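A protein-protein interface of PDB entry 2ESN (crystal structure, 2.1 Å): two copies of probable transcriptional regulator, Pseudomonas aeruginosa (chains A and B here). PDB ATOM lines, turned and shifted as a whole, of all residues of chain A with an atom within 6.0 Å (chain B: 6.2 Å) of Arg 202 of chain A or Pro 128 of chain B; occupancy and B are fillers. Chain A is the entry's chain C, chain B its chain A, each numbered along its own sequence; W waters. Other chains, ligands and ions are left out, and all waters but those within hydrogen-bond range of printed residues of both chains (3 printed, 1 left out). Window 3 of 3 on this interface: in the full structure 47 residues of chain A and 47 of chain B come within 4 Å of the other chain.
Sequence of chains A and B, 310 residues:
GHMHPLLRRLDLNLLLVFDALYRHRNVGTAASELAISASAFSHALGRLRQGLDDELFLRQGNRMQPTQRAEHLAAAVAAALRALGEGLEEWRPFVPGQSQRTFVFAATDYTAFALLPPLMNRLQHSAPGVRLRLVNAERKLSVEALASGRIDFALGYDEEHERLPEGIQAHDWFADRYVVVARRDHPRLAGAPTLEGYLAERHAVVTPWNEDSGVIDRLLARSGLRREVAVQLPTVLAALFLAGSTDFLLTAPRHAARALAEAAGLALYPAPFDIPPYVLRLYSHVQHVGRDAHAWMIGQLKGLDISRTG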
ATOM      1  N   TYR A 198     -31.012 -14.131   9.120  1.00  0.00           N
ATOM      2  CA  TYR A 198     -30.712 -13.863  10.550  1.00  0.00           C
ATOM      3  C   TYR A 198     -30.550 -15.164  11.312  1.00  0.00           C
ATOM      4  O   TYR A 198     -29.551 -15.366  11.939  1.00  0.00           O
ATOM      5  CB  TYR A 198     -31.841 -13.040  11.169  1.00  0.00           C
ATOM      6  CG  TYR A 198     -31.698 -12.675  12.661  1.00  0.00           C
ATOM      7  CD1 TYR A 198     -31.044 -11.500  13.055  1.00  0.00           C
ATOM      8  CD2 TYR A 198     -32.284 -13.462  13.649  1.00  0.00           C
ATOM      9  CE1 TYR A 198     -30.930 -11.134  14.429  1.00  0.00           C
ATOM     10  CE2 TYR A 198     -32.202 -13.111  15.002  1.00  0.00           C
ATOM     11  CZ  TYR A 198     -31.529 -11.941  15.398  1.00  0.00           C
ATOM     12  OH  TYR A 198     -31.441 -11.619  16.763  1.00  0.00           O
ATOM     13  N   ALA A 200     -29.714 -18.044  10.130  1.00  0.00           N
ATOM     14  CA  ALA A 200     -28.607 -18.843   9.593  1.00  0.00           C
ATOM     15  C   ALA A 200     -27.236 -18.525  10.192  1.00  0.00           C
ATOM     16  O   ALA A 200     -26.268 -19.290   9.988  1.00  0.00           O
ATOM     17  CB  ALA A 200     -28.509 -18.683   8.058  1.00  0.00           C
ATOM     18  N   GLU A 201     -27.123 -17.344  10.812  1.00  0.00           N
ATOM     19  CA  GLU A 201     -25.874 -16.881  11.402  1.00  0.00           C
ATOM     20  C   GLU A 201     -25.783 -17.311  12.861  1.00  0.00           C
ATOM     21  O   GLU A 201     -26.783 -17.772  13.448  1.00  0.00           O
ATOM     22  CB  GLU A 201     -25.804 -15.337  11.355  1.00  0.00           C
ATOM     23  CG  GLU A 201     -25.865 -14.782   9.956  1.00  0.00           C
ATOM     24  CD  GLU A 201     -24.675 -15.227   9.053  1.00  0.00           C
ATOM     25  OE1 GLU A 201     -23.564 -15.553   9.571  1.00  0.00           O
ATOM     26  OE2 GLU A 201     -24.867 -15.219   7.795  1.00  0.00           O
ATOM     27  N   ARG A 202     -24.567 -17.200  13.420  1.00  0.00           N
ATOM     28  CA  ARG A 202     -24.344 -17.343  14.868  1.00  0.00           C
ATOM     29  C   ARG A 202     -24.389 -15.959  15.475  1.00  0.00           C
ATOM     30  O   ARG A 202     -23.979 -14.979  14.836  1.00  0.00           O
ATOM     31  CB  ARG A 202     -23.002 -18.009  15.162  1.00  0.00           C
ATOM     32  CG  ARG A 202     -22.891 -19.441  14.584  1.00  0.00           C
ATOM     33  CD  ARG A 202     -21.543 -20.010  14.908  1.00  0.00           C
ATOM     34  NE  ARG A 202     -21.428 -20.551  16.274  1.00  0.00           N
ATOM     35  CZ  ARG A 202     -20.263 -20.617  16.912  1.00  0.00           C
ATOM     36  NH1 ARG A 202     -19.147 -20.136  16.324  1.00  0.00           N
ATOM     37  NH2 ARG A 202     -20.213 -21.100  18.130  1.00  0.00           N
ATOM     38  N   HIS A 203     -24.847 -15.907  16.718  1.00  0.00           N
ATOM     39  CA  HIS A 203     -25.175 -14.689  17.383  1.00  0.00           C
ATOM     40  C   HIS A 203     -24.385 -14.412  18.641  1.00  0.00           C
ATOM     41  O   HIS A 203     -24.058 -15.303  19.440  1.00  0.00           O
ATOM     42  CB  HIS A 203     -26.649 -14.715  17.752  1.00  0.00           C
ATOM     43  CG  HIS A 203     -27.533 -14.755  16.555  1.00  0.00           C
ATOM     44  ND1 HIS A 203     -28.128 -13.632  16.036  1.00  0.00           N
ATOM     45  CD2 HIS A 203     -27.872 -15.788  15.734  1.00  0.00           C
ATOM     46  CE1 HIS A 203     -28.796 -13.969  14.940  1.00  0.00           C
ATOM     47  NE2 HIS A 203     -28.653 -15.269  14.732  1.00  0.00           N
ATOM     48  N   ALA A 204     -24.151 -13.145  18.834  1.00  0.00           N
ATOM     49  CA  ALA A 204     -23.637 -12.658  20.148  1.00  0.00           C
ATOM     50  C   ALA A 204     -24.862 -12.196  20.890  1.00  0.00           C
ATOM     51  O   ALA A 204     -25.737 -11.480  20.348  1.00  0.00           O
ATOM     52  CB  ALA A 204     -22.673 -11.466  19.930  1.00  0.00           C
ATOM     53  N   GLU A 228     -29.042 -19.561  16.927  1.00  0.00           N
ATOM     54  CA  GLU A 228     -27.779 -20.140  17.361  1.00  0.00           C
ATOM     55  C   GLU A 228     -26.867 -19.120  18.048  1.00  0.00           C
ATOM     56  O   GLU A 228     -26.437 -18.149  17.431  1.00  0.00           O
ATOM     57  CB  GLU A 228     -26.991 -20.701  16.175  1.00  0.00           C
ATOM     58  CG  GLU A 228     -26.239 -21.927  16.617  1.00  0.00           C
ATOM     59  CD  GLU A 228     -25.192 -22.362  15.636  1.00  0.00           C
ATOM     60  OE1 GLU A 228     -25.429 -22.200  14.409  1.00  0.00           O
ATOM     61  OE2 GLU A 228     -24.146 -22.867  16.108  1.00  0.00           O
ATOM     62  N   VAL A 229     -26.503 -19.429  19.290  1.00  0.00           N
ATOM     63  CA  VAL A 229     -25.730 -18.524  20.121  1.00  0.00           C
ATOM     64  C   VAL A 229     -24.260 -18.931  20.113  1.00  0.00           C
ATOM     65  O   VAL A 229     -23.932 -20.015  20.510  1.00  0.00           O
ATOM     66  CB  VAL A 229     -26.400 -18.449  21.542  1.00  0.00           C
ATOM     67  CG1 VAL A 229     -25.590 -17.589  22.548  1.00  0.00           C
ATOM     68  CG2 VAL A 229     -27.817 -17.906  21.348  1.00  0.00           C
ATOM     69  N   ALA A 230     -23.381 -18.067  19.640  1.00  0.00           N
ATOM     70  CA  ALA A 230     -21.942 -18.306  19.741  1.00  0.00           C
ATOM     71  C   ALA A 230     -21.362 -17.762  21.087  1.00  0.00           C
ATOM     72  O   ALA A 230     -20.614 -18.439  21.728  1.00  0.00           O
ATOM     73  CB  ALA A 230     -21.201 -17.682  18.537  1.00  0.00           C
ATOM     74  N   VAL A 231     -21.749 -16.558  21.521  1.00  0.00           N
ATOM     75  CA  VAL A 231     -21.137 -15.952  22.743  1.00  0.00           C
ATOM     76  C   VAL A 231     -22.226 -15.286  23.537  1.00  0.00           C
ATOM     77  O   VAL A 231     -23.061 -14.621  22.954  1.00  0.00           O
ATOM     78  CB  VAL A 231     -20.116 -14.904  22.377  1.00  0.00           C
ATOM     79  CG1 VAL A 231     -19.545 -14.224  23.666  1.00  0.00           C
ATOM     80  CG2 VAL A 231     -18.982 -15.496  21.394  1.00  0.00           C
ATOM     81  N   ASP A 247     -18.065 -12.770  12.198  1.00  0.00           N
ATOM     82  CA  ASP A 247     -19.269 -12.825  11.347  1.00  0.00           C
ATOM     83  C   ASP A 247     -20.551 -12.985  12.132  1.00  0.00           C
ATOM     84  O   ASP A 247     -21.644 -13.149  11.551  1.00  0.00           O
ATOM     85  CB  ASP A 247     -19.120 -13.878  10.242  1.00  0.00           C
ATOM     86  CG  ASP A 247     -17.963 -13.572   9.277  1.00  0.00           C
ATOM     87  OD1 ASP A 247     -17.456 -12.434   9.213  1.00  0.00           O
ATOM     88  OD2 ASP A 247     -17.522 -14.499   8.577  1.00  0.00           O
ATOM     89  N   PHE A 248     -20.448 -12.815  13.466  1.00  0.00           N
ATOM     90  CA  PHE A 248     -21.615 -12.899  14.363  1.00  0.00           C
ATOM     91  C   PHE A 248     -22.532 -11.703  14.241  1.00  0.00           C
ATOM     92  O   PHE A 248     -22.098 -10.547  13.994  1.00  0.00           O
ATOM     93  CB  PHE A 248     -21.199 -13.050  15.862  1.00  0.00           C
ATOM     94  CG  PHE A 248     -20.270 -14.215  16.137  1.00  0.00           C
ATOM     95  CD1 PHE A 248     -20.272 -15.338  15.325  1.00  0.00           C
ATOM     96  CD2 PHE A 248     -19.433 -14.208  17.270  1.00  0.00           C
ATOM     97  CE1 PHE A 248     -19.428 -16.449  15.583  1.00  0.00           C
ATOM     98  CE2 PHE A 248     -18.610 -15.340  17.563  1.00  0.00           C
ATOM     99  CZ  PHE A 248     -18.592 -16.440  16.714  1.00  0.00           C
ATOM    100  N   LEU A 249     -23.813 -11.979  14.417  1.00  0.00           N
ATOM    101  CA  LEU A 249     -24.791 -10.927  14.496  1.00  0.00           C
ATOM    102  C   LEU A 249     -25.073 -10.538  15.973  1.00  0.00           C
ATOM    103  O   LEU A 249     -25.164 -11.431  16.833  1.00  0.00           O
ATOM    104  CB  LEU A 249     -26.094 -11.396  13.812  1.00  0.00           C
ATOM    105  CG  LEU A 249     -26.067 -11.650  12.265  1.00  0.00           C
ATOM    106  CD1 LEU A 249     -27.512 -11.626  11.689  1.00  0.00           C
ATOM    107  CD2 LEU A 249     -25.207 -10.685  11.545  1.00  0.00           C
ATOM    108  N   PRO B  96     -11.344 -29.892  18.716  1.00  0.00           N
ATOM    109  CA  PRO B  96     -11.576 -28.491  18.334  1.00  0.00           C
ATOM    110  C   PRO B  96     -12.640 -28.269  17.260  1.00  0.00           C
ATOM    111  O   PRO B  96     -13.632 -27.547  17.486  1.00  0.00           O
ATOM    112  CB  PRO B  96     -10.199 -28.043  17.823  1.00  0.00           C
ATOM    113  CG  PRO B  96      -9.220 -28.875  18.608  1.00  0.00           C
ATOM    114  CD  PRO B  96      -9.938 -30.121  19.101  1.00  0.00           C
ATOM    115  N   GLY B  97     -12.432 -28.904  16.107  1.00  0.00           N
ATOM    116  CA  GLY B  97     -13.193 -28.621  14.924  1.00  0.00           C
ATOM    117  C   GLY B  97     -14.578 -29.184  15.038  1.00  0.00           C
ATOM    118  O   GLY B  97     -15.453 -28.788  14.284  1.00  0.00           O
ATOM    119  N   GLN B  98     -14.798 -30.094  15.984  1.00  0.00           N
ATOM    120  CA  GLN B  98     -16.144 -30.684  16.143  1.00  0.00           C
ATOM    121  C   GLN B  98     -16.897 -30.309  17.413  1.00  0.00           C
ATOM    122  O   GLN B  98     -18.105 -30.446  17.461  1.00  0.00           O
ATOM    123  CB  GLN B  98     -16.079 -32.219  16.047  1.00  0.00           C
ATOM    124  CG  GLN B  98     -16.974 -32.778  14.938  1.00  0.00           C
ATOM    125  CD  GLN B  98     -16.415 -32.431  13.588  1.00  0.00           C
ATOM    126  OE1 GLN B  98     -15.188 -32.354  13.420  1.00  0.00           O
ATOM    127  NE2 GLN B  98     -17.304 -32.193  12.608  1.00  0.00           N
ATOM    128  N   SER B  99     -16.179 -29.867  18.439  1.00  0.00           N
ATOM    129  CA  SER B  99     -16.796 -29.575  19.744  1.00  0.00           C
ATOM    130  C   SER B  99     -17.947 -28.572  19.732  1.00  0.00           C
ATOM    131  O   SER B  99     -17.917 -27.540  19.034  1.00  0.00           O
ATOM    132  CB  SER B  99     -15.754 -29.118  20.747  1.00  0.00           C
ATOM    133  OG  SER B  99     -16.356 -29.008  22.022  1.00  0.00           O
ATOM    134  N   GLN B 100     -18.983 -28.912  20.486  1.00  0.00           N
ATOM    135  CA  GLN B 100     -20.127 -28.028  20.657  1.00  0.00           C
ATOM    136  C   GLN B 100     -20.056 -27.476  22.058  1.00  0.00           C
ATOM    137  O   GLN B 100     -21.033 -26.954  22.566  1.00  0.00           O
ATOM    138  CB  GLN B 100     -21.465 -28.751  20.472  1.00  0.00           C
ATOM    139  CG  GLN B 100     -21.658 -29.463  19.134  1.00  0.00           C
ATOM    140  CD  GLN B 100     -21.582 -28.537  17.982  1.00  0.00           C
ATOM    141  OE1 GLN B 100     -22.493 -27.691  17.859  1.00  0.00           O
ATOM    142  NE2 GLN B 100     -20.601 -28.644  17.200  1.00  0.00           N
ATOM    143  N   MET B 120     -12.287 -14.838  19.048  1.00  0.00           N
ATOM    144  CA  MET B 120     -13.408 -15.352  18.244  1.00  0.00           C
ATOM    145  C   MET B 120     -13.301 -15.064  16.740  1.00  0.00           C
ATOM    146  O   MET B 120     -13.950 -15.734  15.940  1.00  0.00           O
ATOM    147  CB  MET B 120     -14.741 -14.842  18.777  1.00  0.00           C
ATOM    148  CG  MET B 120     -15.025 -15.181  20.244  1.00  0.00           C
ATOM    149  SD  MET B 120     -14.956 -16.859  20.806  1.00  0.00           S
ATOM    150  CE  MET B 120     -16.154 -17.582  19.835  1.00  0.00           C
ATOM    151  N   LEU B 123     -11.513 -18.438  16.480  1.00  0.00           N
ATOM    152  CA  LEU B 123     -12.335 -19.566  16.879  1.00  0.00           C
ATOM    153  C   LEU B 123     -13.585 -19.766  16.035  1.00  0.00           C
ATOM    154  O   LEU B 123     -14.096 -20.867  15.990  1.00  0.00           O
ATOM    155  CB  LEU B 123     -12.733 -19.506  18.343  1.00  0.00           C
ATOM    156  CG  LEU B 123     -11.606 -19.652  19.361  1.00  0.00           C
ATOM    157  CD1 LEU B 123     -12.145 -20.085  20.724  1.00  0.00           C
ATOM    158  CD2 LEU B 123     -10.535 -20.583  18.896  1.00  0.00           C
ATOM    159  N   GLN B 124     -14.088 -18.731  15.387  1.00  0.00           N
ATOM    160  CA  GLN B 124     -15.338 -18.886  14.617  1.00  0.00           C
ATOM    161  C   GLN B 124     -15.168 -19.826  13.381  1.00  0.00           C
ATOM    162  O   GLN B 124     -16.121 -20.472  12.920  1.00  0.00           O
ATOM    163  CB  GLN B 124     -15.874 -17.536  14.172  1.00  0.00           C
ATOM    164  CG  GLN B 124     -14.981 -16.849  13.154  1.00  0.00           C
ATOM    165  CD  GLN B 124     -15.548 -15.535  12.633  1.00  0.00           C
ATOM    166  OE1 GLN B 124     -16.771 -15.320  12.576  1.00  0.00           O
ATOM    167  NE2 GLN B 124     -14.647 -14.628  12.300  1.00  0.00           N
ATOM    168  N   HIS B 125     -13.952 -19.832  12.851  1.00  0.00           N
ATOM    169  CA  HIS B 125     -13.565 -20.639  11.684  1.00  0.00           C
ATOM    170  C   HIS B 125     -12.914 -21.912  12.225  1.00  0.00           C
ATOM    171  O   HIS B 125     -13.309 -22.991  11.827  1.00  0.00           O
ATOM    172  CB  HIS B 125     -12.552 -19.883  10.793  1.00  0.00           C
ATOM    173  CG  HIS B 125     -13.081 -18.596  10.215  1.00  0.00           C
ATOM    174  ND1 HIS B 125     -14.276 -18.523   9.514  1.00  0.00           N
ATOM    175  CD2 HIS B 125     -12.594 -17.325  10.253  1.00  0.00           C
ATOM    176  CE1 HIS B 125     -14.479 -17.276   9.115  1.00  0.00           C
ATOM    177  NE2 HIS B 125     -13.478 -16.529   9.558  1.00  0.00           N
ATOM    178  N   SER B 126     -11.975 -21.779  13.178  1.00  0.00           N
ATOM    179  CA  SER B 126     -11.233 -22.963  13.763  1.00  0.00           C
ATOM    180  C   SER B 126     -12.034 -23.961  14.616  1.00  0.00           C
ATOM    181  O   SER B 126     -11.752 -25.168  14.621  1.00  0.00           O
ATOM    182  CB  SER B 126      -9.961 -22.539  14.512  1.00  0.00           C
ATOM    183  OG  SER B 126     -10.196 -22.195  15.885  1.00  0.00           O
ATOM    184  N   ALA B 127     -13.034 -23.462  15.348  1.00  0.00           N
ATOM    185  CA  ALA B 127     -13.846 -24.313  16.175  1.00  0.00           C
ATOM    186  C   ALA B 127     -15.276 -23.794  16.081  1.00  0.00           C
ATOM    187  O   ALA B 127     -15.808 -23.183  17.039  1.00  0.00           O
ATOM    188  CB  ALA B 127     -13.308 -24.296  17.618  1.00  0.00           C
ATOM    189  N   PRO B 128     -15.910 -24.000  14.908  1.00  0.00           N
ATOM    190  CA  PRO B 128     -17.184 -23.303  14.659  1.00  0.00           C
ATOM    191  C   PRO B 128     -18.335 -23.661  15.567  1.00  0.00           C
ATOM    192  O   PRO B 128     -19.384 -23.039  15.454  1.00  0.00           O
ATOM    193  CB  PRO B 128     -17.561 -23.704  13.208  1.00  0.00           C
ATOM    194  CG  PRO B 128     -16.363 -24.345  12.618  1.00  0.00           C
ATOM    195  CD  PRO B 128     -15.504 -24.862  13.776  1.00  0.00           C
ATOM    196  N   GLY B 129     -18.201 -24.678  16.424  1.00  0.00           N
ATOM    197  CA  GLY B 129     -19.329 -25.061  17.295  1.00  0.00           C
ATOM    198  C   GLY B 129     -19.088 -24.733  18.781  1.00  0.00           C
ATOM    199  O   GLY B 129     -19.977 -24.832  19.586  1.00  0.00           O
ATOM    200  N   VAL B 130     -17.862 -24.386  19.133  1.00  0.00           N
ATOM    201  CA  VAL B 130     -17.468 -23.947  20.515  1.00  0.00           C
ATOM    202  C   VAL B 130     -18.102 -22.575  20.855  1.00  0.00           C
ATOM    203  O   VAL B 130     -18.042 -21.627  20.034  1.00  0.00           O
ATOM    204  CB  VAL B 130     -15.919 -23.869  20.584  1.00  0.00           C
ATOM    205  CG1 VAL B 130     -15.400 -22.968  21.753  1.00  0.00           C
ATOM    206  CG2 VAL B 130     -15.266 -25.327  20.608  1.00  0.00           C
ATOM    207  N   ARG B 131     -18.749 -22.492  22.016  1.00  0.00           N
ATOM    208  CA  ARG B 131     -19.395 -21.261  22.503  1.00  0.00           C
ATOM    209  C   ARG B 131     -18.615 -20.714  23.686  1.00  0.00           C
ATOM    210  O   ARG B 131     -17.907 -21.462  24.345  1.00  0.00           O
ATOM    211  CB  ARG B 131     -20.831 -21.529  22.971  1.00  0.00           C
ATOM    212  CG  ARG B 131     -21.817 -21.930  21.867  1.00  0.00           C
ATOM    213  CD  ARG B 131     -23.135 -22.484  22.486  1.00  0.00           C
ATOM    214  NE  ARG B 131     -24.109 -21.439  22.900  1.00  0.00           N
ATOM    215  CZ  ARG B 131     -24.417 -21.120  24.160  1.00  0.00           C
ATOM    216  NH1 ARG B 131     -25.327 -20.193  24.400  1.00  0.00           N
ATOM    217  NH2 ARG B 131     -23.840 -21.732  25.189  1.00  0.00           N
HETATM  218  O   HOH W   1     -18.449 -19.757  13.289  1.00  0.00           O
HETATM  219  O   HOH W   2     -15.024 -12.177  10.608  1.00  0.00           O
HETATM  220  O   HOH W   3     -22.053 -23.818  14.754  1.00  0.00           O
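N of Asp 247 of chain A sits at hydrogen-bond distance from OE1 of Gln 124 of chain B (2.9 Å).
NH1 of Arg 202 of chain A sits close to O of Pro 128 of chain B, 3.0 Å away.
The guanidinium group of Arg 202 of chain A lies within hydrogen-bond range of the backbone carbonyl oxygen of Val 130 of chain B (2.9 Å).
The guanidinium group (NE) of Arg 131 of chain B is in hydrogen-bond range of the backbone carbonyl oxygen (O) of Val 229 of chain A (2.8 Å).
The backbone NH (N) of Val 130 of chain B sits at hydrogen-bond distance from the backbone carbonyl oxygen (O) of Ser 99 of chain B (3.2 Å).
NE of Arg 202 of chain A lies within salt-bridge range of OE2 of Glu 228 of chain A (3.6 Å).
The backbone carbonyl oxygen (O) of Arg 202 of chain A is in hydrogen-bond range of the backbone NH (N) of Leu 249 of chain A (3.0 Å).
The backbone carbonyl oxygen (O) of His 203 of chain A sits at hydrogen-bond distance from the backbone NH (N) of Ala 230 of chain A, at 2.9 Å.
The backbone carbonyl oxygen (O) of His 203 of chain A sits at hydrogen-bond distance from the backbone NH (N) of Val 231 of chain A, at 3.4 Å.
Arg 202 of chain A touches Gly 129 of chain B.
Ala 230 of chain A touches Arg 131 of chain B (O to CA, 3.2 Å).
Val 231 of chain A touches Met 120 of chain B.
Phe 248 of chain A touches Gln 124 of chain B (CZ to CB, 3.9 Å).
Of the printed residues of chain B, Arg 202 of chain A touches Pro 128 (3.0 Å), Gly 129 (3.9 Å) and Val 130 (2.9 Å).
Of the printed residues of chain B, Phe 248 of chain A touches Gln 124 (3.9 Å).
Of the printed residues of chain A, Gln 124 of chain B touches Asp 247 and Phe 248.
Ser 126 of chain B touches none of the printed residues of chain A.
Of the printed residues of chain A, Gly 129 of chain B touches Arg 202.
The nearest printed residue of chain B that does not touch Arg 202 of chain A is Arg 131 of chain B (4.2 Å).
The nearest printed residue of chain A that does not touch Arg 131 of chain B is Arg 202 of chain A (4.2 Å).
Of the 13 printed residues of chain A, 6 touch a printed residue of chain B.
Hydrophobic or aromatic side chains of chain A that line the printed part of chain B: Val 229, Val 231 and Phe 248.
Among the printed residues, no Asp or Glu carboxylate lies within 4 Å of a Lys or Arg side-chain nitrogen of the other chain.
No position is printed for both chains.
Of the 8 pairs that touch across the chains among the printed residues, none has its exchanged pair printed and touching as well.
Water W1 lies within hydrogen-bond range of the backbone carbonyl oxygen (O) of Gln 124 of chain B (2.5 Å) and the guanidinium group (NH1) of Arg 202 of chain A (3.1 Å).
Water W3 lies within hydrogen-bond range of the side-chain carboxylate (OE2) of Glu 228 of chain A (2.7 Å) and the backbone carbonyl oxygen (O) of Pro 128 of chain B (2.9 Å).
Water W2 lies within hydrogen-bond range of the side-chain carboxylate of Asp 247 of chain A and the side-chain amide nitrogen of Gln 124 of chain B.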
